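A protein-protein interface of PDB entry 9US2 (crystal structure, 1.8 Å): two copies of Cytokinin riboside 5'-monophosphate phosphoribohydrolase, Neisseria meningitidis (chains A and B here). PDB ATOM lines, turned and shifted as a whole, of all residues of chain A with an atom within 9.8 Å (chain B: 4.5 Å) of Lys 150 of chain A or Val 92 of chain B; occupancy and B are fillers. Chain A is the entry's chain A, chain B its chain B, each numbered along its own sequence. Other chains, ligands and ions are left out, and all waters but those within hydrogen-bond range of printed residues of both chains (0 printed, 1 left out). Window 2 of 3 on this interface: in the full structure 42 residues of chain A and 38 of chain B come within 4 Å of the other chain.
The backbone carbonyl oxygen of Val 92 of chain B is in hydrogen-bond range of the side-chain amino group of Lys 150 of chain A, at 2.8 Å. NZ of Lys 150 of chain A lies within hydrogen-bond range of O of Ser 110 of chain B (2.8 Å).
OG1 of Thr 148 of chain A is in hydrogen-bond range of O of Leu 145 of chain A, at 3.5 Å. The backbone carbonyl oxygen (O) of Leu 145 of chain A sits at hydrogen-bond distance from the backbone NH (N) of Val 151 of chain A (3.3 Å). The backbone NH (N) of Val 92 of chain B sits at hydrogen-bond distance from the backbone carbonyl oxygen (O) of Phe 109 of chain B (3.0 Å). The backbone NH of Lys 150 of chain A lies within hydrogen-bond range of the backbone carbonyl oxygen of Leu 145 of chain A (2.9 Å). The backbone carbonyl oxygen (O) of Thr 144 of chain A is in hydrogen-bond range of the side-chain hydroxyl (OG1) of Thr 148 of chain A, at 2.8 Å.
Among the printed residues, pairs that only touch across the chains: Thr 144 of chain A with Phe 112 of chain B, Leu 145 of chain A with Phe 112 of chain B, Thr 148 of chain A with Pro 94 of chain B, Thr 148 of chain A with Phe 112 of chain B and Gly 149 of chain A with Pro 94 of chain B.
Of the printed residues of chain B, Thr 144 of chain A touches Phe 112 (3.999 Å). Printed residues of chain B within 4 Å of Leu 145 of chain A: Phe 112 (3.8 Å). Lys 150 of chain A touches just these residues of chain B: Val 92 and Ser 110. No residue of chain A comes within 4 Å of Ile 91 of chain B. Of chain A, only Lys 150 comes within 4 Å of Val 92 of chain B. Of the printed residues of chain A, Ser 110 of chain B touches Lys 150. The nearest residue of chain A that does not touch Val 92 of chain B is Thr 148 of chain A (7.1 Å). The nearest printed residue of chain B that does not touch Leu 145 of chain A is Pro 94 of chain B (7.1 Å).
Printed residues of chain B that touch a printed residue of chain A: Val 92, Pro 94, Ser 110 and Phe 112. Hydrophobic or aromatic side chains of chain A within 4 Å of the printed part of chain B: Leu 145. Among the printed residues, 7 pairs touch across the chains.
No position is printed for both chains. Of the 7 pairs that touch across the chains among the printed residues, none has its exchanged pair printed and touching as well.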
ATOM      1  N   ALA A 117      23.943  20.423 -16.115  1.00  0.00           N
ATOM      2  CA  ALA A 117      25.265  19.901 -15.746  1.00  0.00           C
ATOM      3  C   ALA A 117      25.271  19.403 -14.313  1.00  0.00           C
ATOM      4  O   ALA A 117      25.913  18.391 -13.987  1.00  0.00           O
ATOM      5  CB  ALA A 117      26.339  20.972 -15.925  1.00  0.00           C
ATOM      6  N   PHE A 120      23.351  16.138 -14.054  1.00  0.00           N
ATOM      7  CA  PHE A 120      24.051  15.007 -14.641  1.00  0.00           C
ATOM      8  C   PHE A 120      25.349  14.687 -13.918  1.00  0.00           C
ATOM      9  O   PHE A 120      25.811  13.543 -13.991  1.00  0.00           O
ATOM     10  CB  PHE A 120      24.321  15.265 -16.119  1.00  0.00           C
ATOM     11  CG  PHE A 120      23.061  15.497 -16.928  1.00  0.00           C
ATOM     12  CD1 PHE A 120      21.872  14.873 -16.574  1.00  0.00           C
ATOM     13  CD2 PHE A 120      23.068  16.330 -18.033  1.00  0.00           C
ATOM     14  CE1 PHE A 120      20.718  15.070 -17.311  1.00  0.00           C
ATOM     15  CE2 PHE A 120      21.907  16.526 -18.777  1.00  0.00           C
ATOM     16  CZ  PHE A 120      20.744  15.900 -18.415  1.00  0.00           C
ATOM     17  N   ARG A 121      25.945  15.656 -13.222  1.00  0.00           N
ATOM     18  CA  ARG A 121      27.161  15.319 -12.480  1.00  0.00           C
ATOM     19  C   ARG A 121      26.853  14.593 -11.178  1.00  0.00           C
ATOM     20  O   ARG A 121      27.629  13.721 -10.773  1.00  0.00           O
ATOM     21  CB  ARG A 121      28.001  16.570 -12.189  1.00  0.00           C
ATOM     22  CG  ARG A 121      29.432  16.229 -11.689  1.00  0.00           C
ATOM     23  CD  ARG A 121      29.756  16.934 -10.384  1.00  0.00           C
ATOM     24  NE  ARG A 121      31.020  16.515  -9.769  1.00  0.00           N
ATOM     25  CZ  ARG A 121      31.185  15.404  -9.056  1.00  0.00           C
ATOM     26  NH1 ARG A 121      30.206  14.522  -8.905  1.00  0.00           N
ATOM     27  NH2 ARG A 121      32.358  15.172  -8.475  1.00  0.00           N
ATOM     28  N   TYR A 126      17.967   8.158 -13.101  1.00  0.00           N
ATOM     29  CA  TYR A 126      16.997   9.127 -13.603  1.00  0.00           C
ATOM     30  C   TYR A 126      15.619   8.484 -13.637  1.00  0.00           C
ATOM     31  O   TYR A 126      15.478   7.347 -14.093  1.00  0.00           O
ATOM     32  CB  TYR A 126      17.392   9.616 -15.006  1.00  0.00           C
ATOM     33  CG  TYR A 126      18.736  10.302 -14.953  1.00  0.00           C
ATOM     34  CD1 TYR A 126      18.825  11.653 -14.619  1.00  0.00           C
ATOM     35  CD2 TYR A 126      19.911   9.583 -15.140  1.00  0.00           C
ATOM     36  CE1 TYR A 126      20.047  12.272 -14.492  1.00  0.00           C
ATOM     37  CE2 TYR A 126      21.156  10.203 -15.040  1.00  0.00           C
ATOM     38  CZ  TYR A 126      21.208  11.548 -14.723  1.00  0.00           C
ATOM     39  OH  TYR A 126      22.421  12.171 -14.613  1.00  0.00           O
ATOM     40  N   GLU A 141      18.758  14.496 -23.827  1.00  0.00           N
ATOM     41  CA  GLU A 141      20.124  14.910 -23.502  1.00  0.00           C
ATOM     42  C   GLU A 141      20.843  13.846 -22.684  1.00  0.00           C
ATOM     43  O   GLU A 141      21.964  13.454 -23.021  1.00  0.00           O
ATOM     44  CB  GLU A 141      20.129  16.246 -22.751  1.00  0.00           C
ATOM     45  CG  GLU A 141      21.524  16.899 -22.712  1.00  0.00           C
ATOM     46  CD  GLU A 141      21.481  18.381 -22.368  1.00  0.00           C
ATOM     47  OE1 GLU A 141      20.600  19.102 -22.902  1.00  0.00           O
ATOM     48  OE2 GLU A 141      22.345  18.832 -21.562  1.00  0.00           O
ATOM     49  N   ILE A 142      20.212  13.330 -21.628  1.00  0.00           N
ATOM     50  CA  ILE A 142      20.913  12.310 -20.848  1.00  0.00           C
ATOM     51  C   ILE A 142      21.096  11.023 -21.666  1.00  0.00           C
ATOM     52  O   ILE A 142      22.138  10.373 -21.577  1.00  0.00           O
ATOM     53  CB  ILE A 142      20.217  12.045 -19.499  1.00  0.00           C
ATOM     54  CG1 ILE A 142      21.095  11.136 -18.606  1.00  0.00           C
ATOM     55  CG2 ILE A 142      18.811  11.436 -19.676  1.00  0.00           C
ATOM     56  CD1 ILE A 142      22.518  11.645 -18.390  1.00  0.00           C
ATOM     57  N   LEU A 143      20.107  10.644 -22.484  1.00  0.00           N
ATOM     58  CA  LEU A 143      20.306   9.494 -23.377  1.00  0.00           C
ATOM     59  C   LEU A 143      21.501   9.708 -24.297  1.00  0.00           C
ATOM     60  O   LEU A 143      22.320   8.795 -24.496  1.00  0.00           O
ATOM     61  CB  LEU A 143      19.054   9.236 -24.209  1.00  0.00           C
ATOM     62  CG  LEU A 143      17.889   8.541 -23.512  1.00  0.00           C
ATOM     63  CD1 LEU A 143      16.597   8.701 -24.306  1.00  0.00           C
ATOM     64  CD2 LEU A 143      18.252   7.049 -23.265  1.00  0.00           C
ATOM     65  N   THR A 144      21.633  10.919 -24.849  1.00  0.00           N
ATOM     66  CA  THR A 144      22.757  11.222 -25.732  1.00  0.00           C
ATOM     67  C   THR A 144      24.085  11.159 -24.989  1.00  0.00           C
ATOM     68  O   THR A 144      25.072  10.613 -25.504  1.00  0.00           O
ATOM     69  CB  THR A 144      22.570  12.603 -26.364  1.00  0.00           C
ATOM     70  OG1 THR A 144      21.408  12.585 -27.201  1.00  0.00           O
ATOM     71  CG2 THR A 144      23.795  12.990 -27.224  1.00  0.00           C
ATOM     72  N   LEU A 145      24.132  11.725 -23.781  1.00  0.00           N
ATOM     73  CA  LEU A 145      25.369  11.717 -23.013  1.00  0.00           C
ATOM     74  C   LEU A 145      25.742  10.292 -22.604  1.00  0.00           C
ATOM     75  O   LEU A 145      26.926   9.944 -22.587  1.00  0.00           O
ATOM     76  CB  LEU A 145      25.225  12.618 -21.777  1.00  0.00           C
ATOM     77  CG  LEU A 145      25.016  14.123 -22.040  1.00  0.00           C
ATOM     78  CD1 LEU A 145      24.553  14.861 -20.775  1.00  0.00           C
ATOM     79  CD2 LEU A 145      26.288  14.770 -22.603  1.00  0.00           C
ATOM     80  N   VAL A 146      24.755   9.447 -22.269  1.00  0.00           N
ATOM     81  CA  VAL A 146      25.084   8.054 -21.936  1.00  0.00           C
ATOM     82  C   VAL A 146      25.502   7.296 -23.195  1.00  0.00           C
ATOM     83  O   VAL A 146      26.547   6.635 -23.224  1.00  0.00           O
ATOM     84  CB  VAL A 146      23.907   7.353 -21.221  1.00  0.00           C
ATOM     85  CG1 VAL A 146      24.157   5.830 -21.102  1.00  0.00           C
ATOM     86  CG2 VAL A 146      23.698   7.921 -19.849  1.00  0.00           C
ATOM     87  N   GLN A 147      24.690   7.376 -24.253  1.00  0.00           N
ATOM     88  CA  GLN A 147      25.043   6.777 -25.540  1.00  0.00           C
ATOM     89  C   GLN A 147      26.480   7.034 -25.979  1.00  0.00           C
ATOM     90  O   GLN A 147      27.184   6.120 -26.423  1.00  0.00           O
ATOM     91  CB  GLN A 147      24.126   7.309 -26.627  1.00  0.00           C
ATOM     92  CG  GLN A 147      23.981   6.369 -27.787  1.00  0.00           C
ATOM     93  CD  GLN A 147      22.836   6.745 -28.664  1.00  0.00           C
ATOM     94  OE1 GLN A 147      22.648   7.924 -28.987  1.00  0.00           O
ATOM     95  NE2 GLN A 147      22.107   5.750 -29.129  1.00  0.00           N
ATOM     96  N   THR A 148      26.909   8.289 -25.920  1.00  0.00           N
ATOM     97  CA  THR A 148      28.207   8.678 -26.444  1.00  0.00           C
ATOM     98  C   THR A 148      29.337   8.468 -25.451  1.00  0.00           C
ATOM     99  O   THR A 148      30.501   8.652 -25.817  1.00  0.00           O
ATOM    100  CB  THR A 148      28.191  10.150 -26.879  1.00  0.00           C
ATOM    101  OG1 THR A 148      27.864  10.980 -25.761  1.00  0.00           O
ATOM    102  CG2 THR A 148      27.182  10.363 -27.965  1.00  0.00           C
ATOM    103  N   GLY A 149      29.027   8.092 -24.212  1.00  0.00           N
ATOM    104  CA  GLY A 149      30.052   7.907 -23.213  1.00  0.00           C
ATOM    105  C   GLY A 149      30.517   9.169 -22.532  1.00  0.00           C
ATOM    106  O   GLY A 149      31.579   9.154 -21.901  1.00  0.00           O
ATOM    107  N   LYS A 150      29.764  10.266 -22.636  1.00  0.00           N
ATOM    108  CA  LYS A 150      30.160  11.475 -21.927  1.00  0.00           C
ATOM    109  C   LYS A 150      29.892  11.363 -20.436  1.00  0.00           C
ATOM    110  O   LYS A 150      30.591  11.999 -19.642  1.00  0.00           O
ATOM    111  CB  LYS A 150      29.438  12.698 -22.501  1.00  0.00           C
ATOM    112  CG  LYS A 150      29.893  13.079 -23.903  1.00  0.00           C
ATOM    113  CD  LYS A 150      31.360  13.424 -23.935  1.00  0.00           C
ATOM    114  CE  LYS A 150      31.686  14.290 -25.138  1.00  0.00           C
ATOM    115  NZ  LYS A 150      32.979  15.015 -24.959  1.00  0.00           N
ATOM    116  N   VAL A 151      28.876  10.599 -20.037  1.00  0.00           N
ATOM    117  CA  VAL A 151      28.643  10.307 -18.622  1.00  0.00           C
ATOM    118  C   VAL A 151      28.551   8.797 -18.451  1.00  0.00           C
ATOM    119  O   VAL A 151      28.226   8.068 -19.400  1.00  0.00           O
ATOM    120  CB  VAL A 151      27.369  11.005 -18.088  1.00  0.00           C
ATOM    121  CG1 VAL A 151      27.414  12.508 -18.368  1.00  0.00           C
ATOM    122  CG2 VAL A 151      26.138  10.385 -18.691  1.00  0.00           C
ATOM    123  N   PRO A 152      28.832   8.295 -17.248  1.00  0.00           N
ATOM    124  CA  PRO A 152      28.821   6.848 -17.037  1.00  0.00           C
ATOM    125  C   PRO A 152      27.434   6.277 -17.239  1.00  0.00           C
ATOM    126  O   PRO A 152      26.420   6.946 -16.968  1.00  0.00           O
ATOM    127  CB  PRO A 152      29.275   6.699 -15.578  1.00  0.00           C
ATOM    128  CG  PRO A 152      30.084   7.913 -15.317  1.00  0.00           C
ATOM    129  CD  PRO A 152      29.423   9.012 -16.102  1.00  0.00           C
ATOM    130  N   PRO A 153      27.341   5.021 -17.674  1.00  0.00           N
ATOM    131  CA  PRO A 153      26.041   4.335 -17.727  1.00  0.00           C
ATOM    132  C   PRO A 153      25.265   4.494 -16.426  1.00  0.00           C
ATOM    133  O   PRO A 153      25.834   4.497 -15.329  1.00  0.00           O
ATOM    134  CB  PRO A 153      26.430   2.872 -17.968  1.00  0.00           C
ATOM    135  CG  PRO A 153      27.762   2.948 -18.630  1.00  0.00           C
ATOM    136  CD  PRO A 153      28.456   4.127 -18.026  1.00  0.00           C
ATOM    137  N   CYS A 154      23.948   4.651 -16.557  1.00  0.00           N
ATOM    138  CA  CYS A 154      23.074   4.790 -15.400  1.00  0.00           C
ATOM    139  C   CYS A 154      21.687   4.353 -15.820  1.00  0.00           C
ATOM    140  O   CYS A 154      21.354   4.427 -17.008  1.00  0.00           O
ATOM    141  CB  CYS A 154      23.022   6.238 -14.911  1.00  0.00           C
ATOM    142  SG  CYS A 154      22.800   7.355 -16.301  1.00  0.00           S
ATOM    143  N   ASN B  90      32.329  20.977 -34.744  1.00  0.00           N
ATOM    144  CA  ASN B  90      32.782  19.596 -34.603  1.00  0.00           C
ATOM    145  C   ASN B  90      32.922  19.223 -33.132  1.00  0.00           C
ATOM    146  O   ASN B  90      33.489  19.983 -32.340  1.00  0.00           O
ATOM    147  CB  ASN B  90      34.129  19.421 -35.312  1.00  0.00           C
ATOM    148  CG  ASN B  90      34.062  19.762 -36.799  1.00  0.00           C
ATOM    149  OD1 ASN B  90      33.574  18.969 -37.608  1.00  0.00           O
ATOM    150  ND2 ASN B  90      34.534  20.965 -37.164  1.00  0.00           N
ATOM    151  N   ILE B  91      32.433  18.035 -32.766  1.00  0.00           N
ATOM    152  CA  ILE B  91      32.345  17.620 -31.367  1.00  0.00           C
ATOM    153  C   ILE B  91      33.385  16.535 -31.102  1.00  0.00           C
ATOM    154  O   ILE B  91      33.624  15.662 -31.945  1.00  0.00           O
ATOM    155  CB  ILE B  91      30.916  17.146 -30.999  1.00  0.00           C
ATOM    156  CG1 ILE B  91      30.812  16.743 -29.522  1.00  0.00           C
ATOM    157  CG2 ILE B  91      30.445  15.971 -31.896  1.00  0.00           C
ATOM    158  CD1 ILE B  91      30.823  17.902 -28.533  1.00  0.00           C
ATOM    159  N   VAL B  92      34.026  16.616 -29.938  1.00  0.00           N
ATOM    160  CA  VAL B  92      35.000  15.626 -29.489  1.00  0.00           C
ATOM    161  C   VAL B  92      34.241  14.516 -28.767  1.00  0.00           C
ATOM    162  O   VAL B  92      33.680  14.727 -27.683  1.00  0.00           O
ATOM    163  CB  VAL B  92      36.059  16.254 -28.574  1.00  0.00           C
ATOM    164  CG1 VAL B  92      37.110  15.230 -28.210  1.00  0.00           C
ATOM    165  CG2 VAL B  92      36.702  17.460 -29.241  1.00  0.00           C
ATOM    166  N   LEU B  93      34.220  13.337 -29.370  1.00  0.00           N
ATOM    167  CA  LEU B  93      33.530  12.184 -28.829  1.00  0.00           C
ATOM    168  C   LEU B  93      34.530  11.089 -28.464  1.00  0.00           C
ATOM    169  O   LEU B  93      35.583  10.964 -29.098  1.00  0.00           O
ATOM    170  CB  LEU B  93      32.512  11.630 -29.836  1.00  0.00           C
ATOM    171  CG  LEU B  93      31.402  12.588 -30.276  1.00  0.00           C
ATOM    172  CD1 LEU B  93      30.572  11.976 -31.363  1.00  0.00           C
ATOM    173  CD2 LEU B  93      30.507  12.912 -29.099  1.00  0.00           C
ATOM    174  N   PRO B  94      34.251  10.312 -27.417  1.00  0.00           N
ATOM    175  CA  PRO B  94      35.097   9.137 -27.140  1.00  0.00           C
ATOM    176  C   PRO B  94      35.248   8.214 -28.346  1.00  0.00           C
ATOM    177  O   PRO B  94      36.360   7.738 -28.618  1.00  0.00           O
ATOM    178  CB  PRO B  94      34.387   8.460 -25.957  1.00  0.00           C
ATOM    179  CG  PRO B  94      33.424   9.506 -25.386  1.00  0.00           C
ATOM    180  CD  PRO B  94      33.456  10.731 -26.251  1.00  0.00           C
ATOM    181  N   ARG B 108      35.813  23.580 -33.148  1.00  0.00           N
ATOM    182  CA  ARG B 108      35.881  22.334 -32.389  1.00  0.00           C
ATOM    183  C   ARG B 108      35.468  22.576 -30.940  1.00  0.00           C
ATOM    184  O   ARG B 108      35.755  23.641 -30.379  1.00  0.00           O
ATOM    185  CB  ARG B 108      37.302  21.732 -32.488  1.00  0.00           C
ATOM    186  CG  ARG B 108      37.516  20.439 -31.726  1.00  0.00           C
ATOM    187  CD  ARG B 108      38.978  19.996 -31.797  1.00  0.00           C
ATOM    188  NE  ARG B 108      39.535  19.737 -30.477  1.00  0.00           N
ATOM    189  CZ  ARG B 108      40.201  18.641 -30.140  1.00  0.00           C
ATOM    190  NH1 ARG B 108      40.409  17.663 -31.008  1.00  0.00           N
ATOM    191  NH2 ARG B 108      40.659  18.516 -28.896  1.00  0.00           N
ATOM    192  N   PHE B 109      34.766  21.598 -30.346  1.00  0.00           N
ATOM    193  CA  PHE B 109      34.230  21.712 -28.988  1.00  0.00           C
ATOM    194  C   PHE B 109      34.448  20.432 -28.198  1.00  0.00           C
ATOM    195  O   PHE B 109      34.200  19.330 -28.701  1.00  0.00           O
ATOM    196  CB  PHE B 109      32.725  22.028 -29.014  1.00  0.00           C
ATOM    197  CG  PHE B 109      32.408  23.287 -29.750  1.00  0.00           C
ATOM    198  CD1 PHE B 109      32.383  24.505 -29.092  1.00  0.00           C
ATOM    199  CD2 PHE B 109      32.176  23.255 -31.116  1.00  0.00           C
ATOM    200  CE1 PHE B 109      32.120  25.672 -29.791  1.00  0.00           C
ATOM    201  CE2 PHE B 109      31.905  24.406 -31.820  1.00  0.00           C
ATOM    202  CZ  PHE B 109      31.884  25.625 -31.165  1.00  0.00           C
ATOM    203  N   SER B 110      34.885  20.583 -26.938  1.00  0.00           N
ATOM    204  CA  SER B 110      35.070  19.412 -26.083  1.00  0.00           C
ATOM    205  C   SER B 110      33.750  18.898 -25.520  1.00  0.00           C
ATOM    206  O   SER B 110      33.642  17.717 -25.185  1.00  0.00           O
ATOM    207  CB  SER B 110      36.033  19.739 -24.937  1.00  0.00           C
ATOM    208  OG  SER B 110      37.265  20.245 -25.424  1.00  0.00           O
ATOM    209  N   PHE B 112      29.212  19.009 -25.483  1.00  0.00           N
ATOM    210  CA  PHE B 112      27.959  19.332 -26.152  1.00  0.00           C
ATOM    211  C   PHE B 112      27.447  20.717 -25.766  1.00  0.00           C
ATOM    212  O   PHE B 112      26.815  21.398 -26.589  1.00  0.00           O
ATOM    213  CB  PHE B 112      26.911  18.263 -25.822  1.00  0.00           C
ATOM    214  CG  PHE B 112      27.050  17.000 -26.629  1.00  0.00           C
ATOM    215  CD1 PHE B 112      26.815  17.003 -27.997  1.00  0.00           C
ATOM    216  CD2 PHE B 112      27.427  15.808 -26.028  1.00  0.00           C
ATOM    217  CE1 PHE B 112      26.934  15.848 -28.749  1.00  0.00           C
ATOM    218  CE2 PHE B 112      27.551  14.642 -26.780  1.00  0.00           C
ATOM    219  CZ  PHE B 112      27.309  14.662 -28.143  1.00  0.00           C
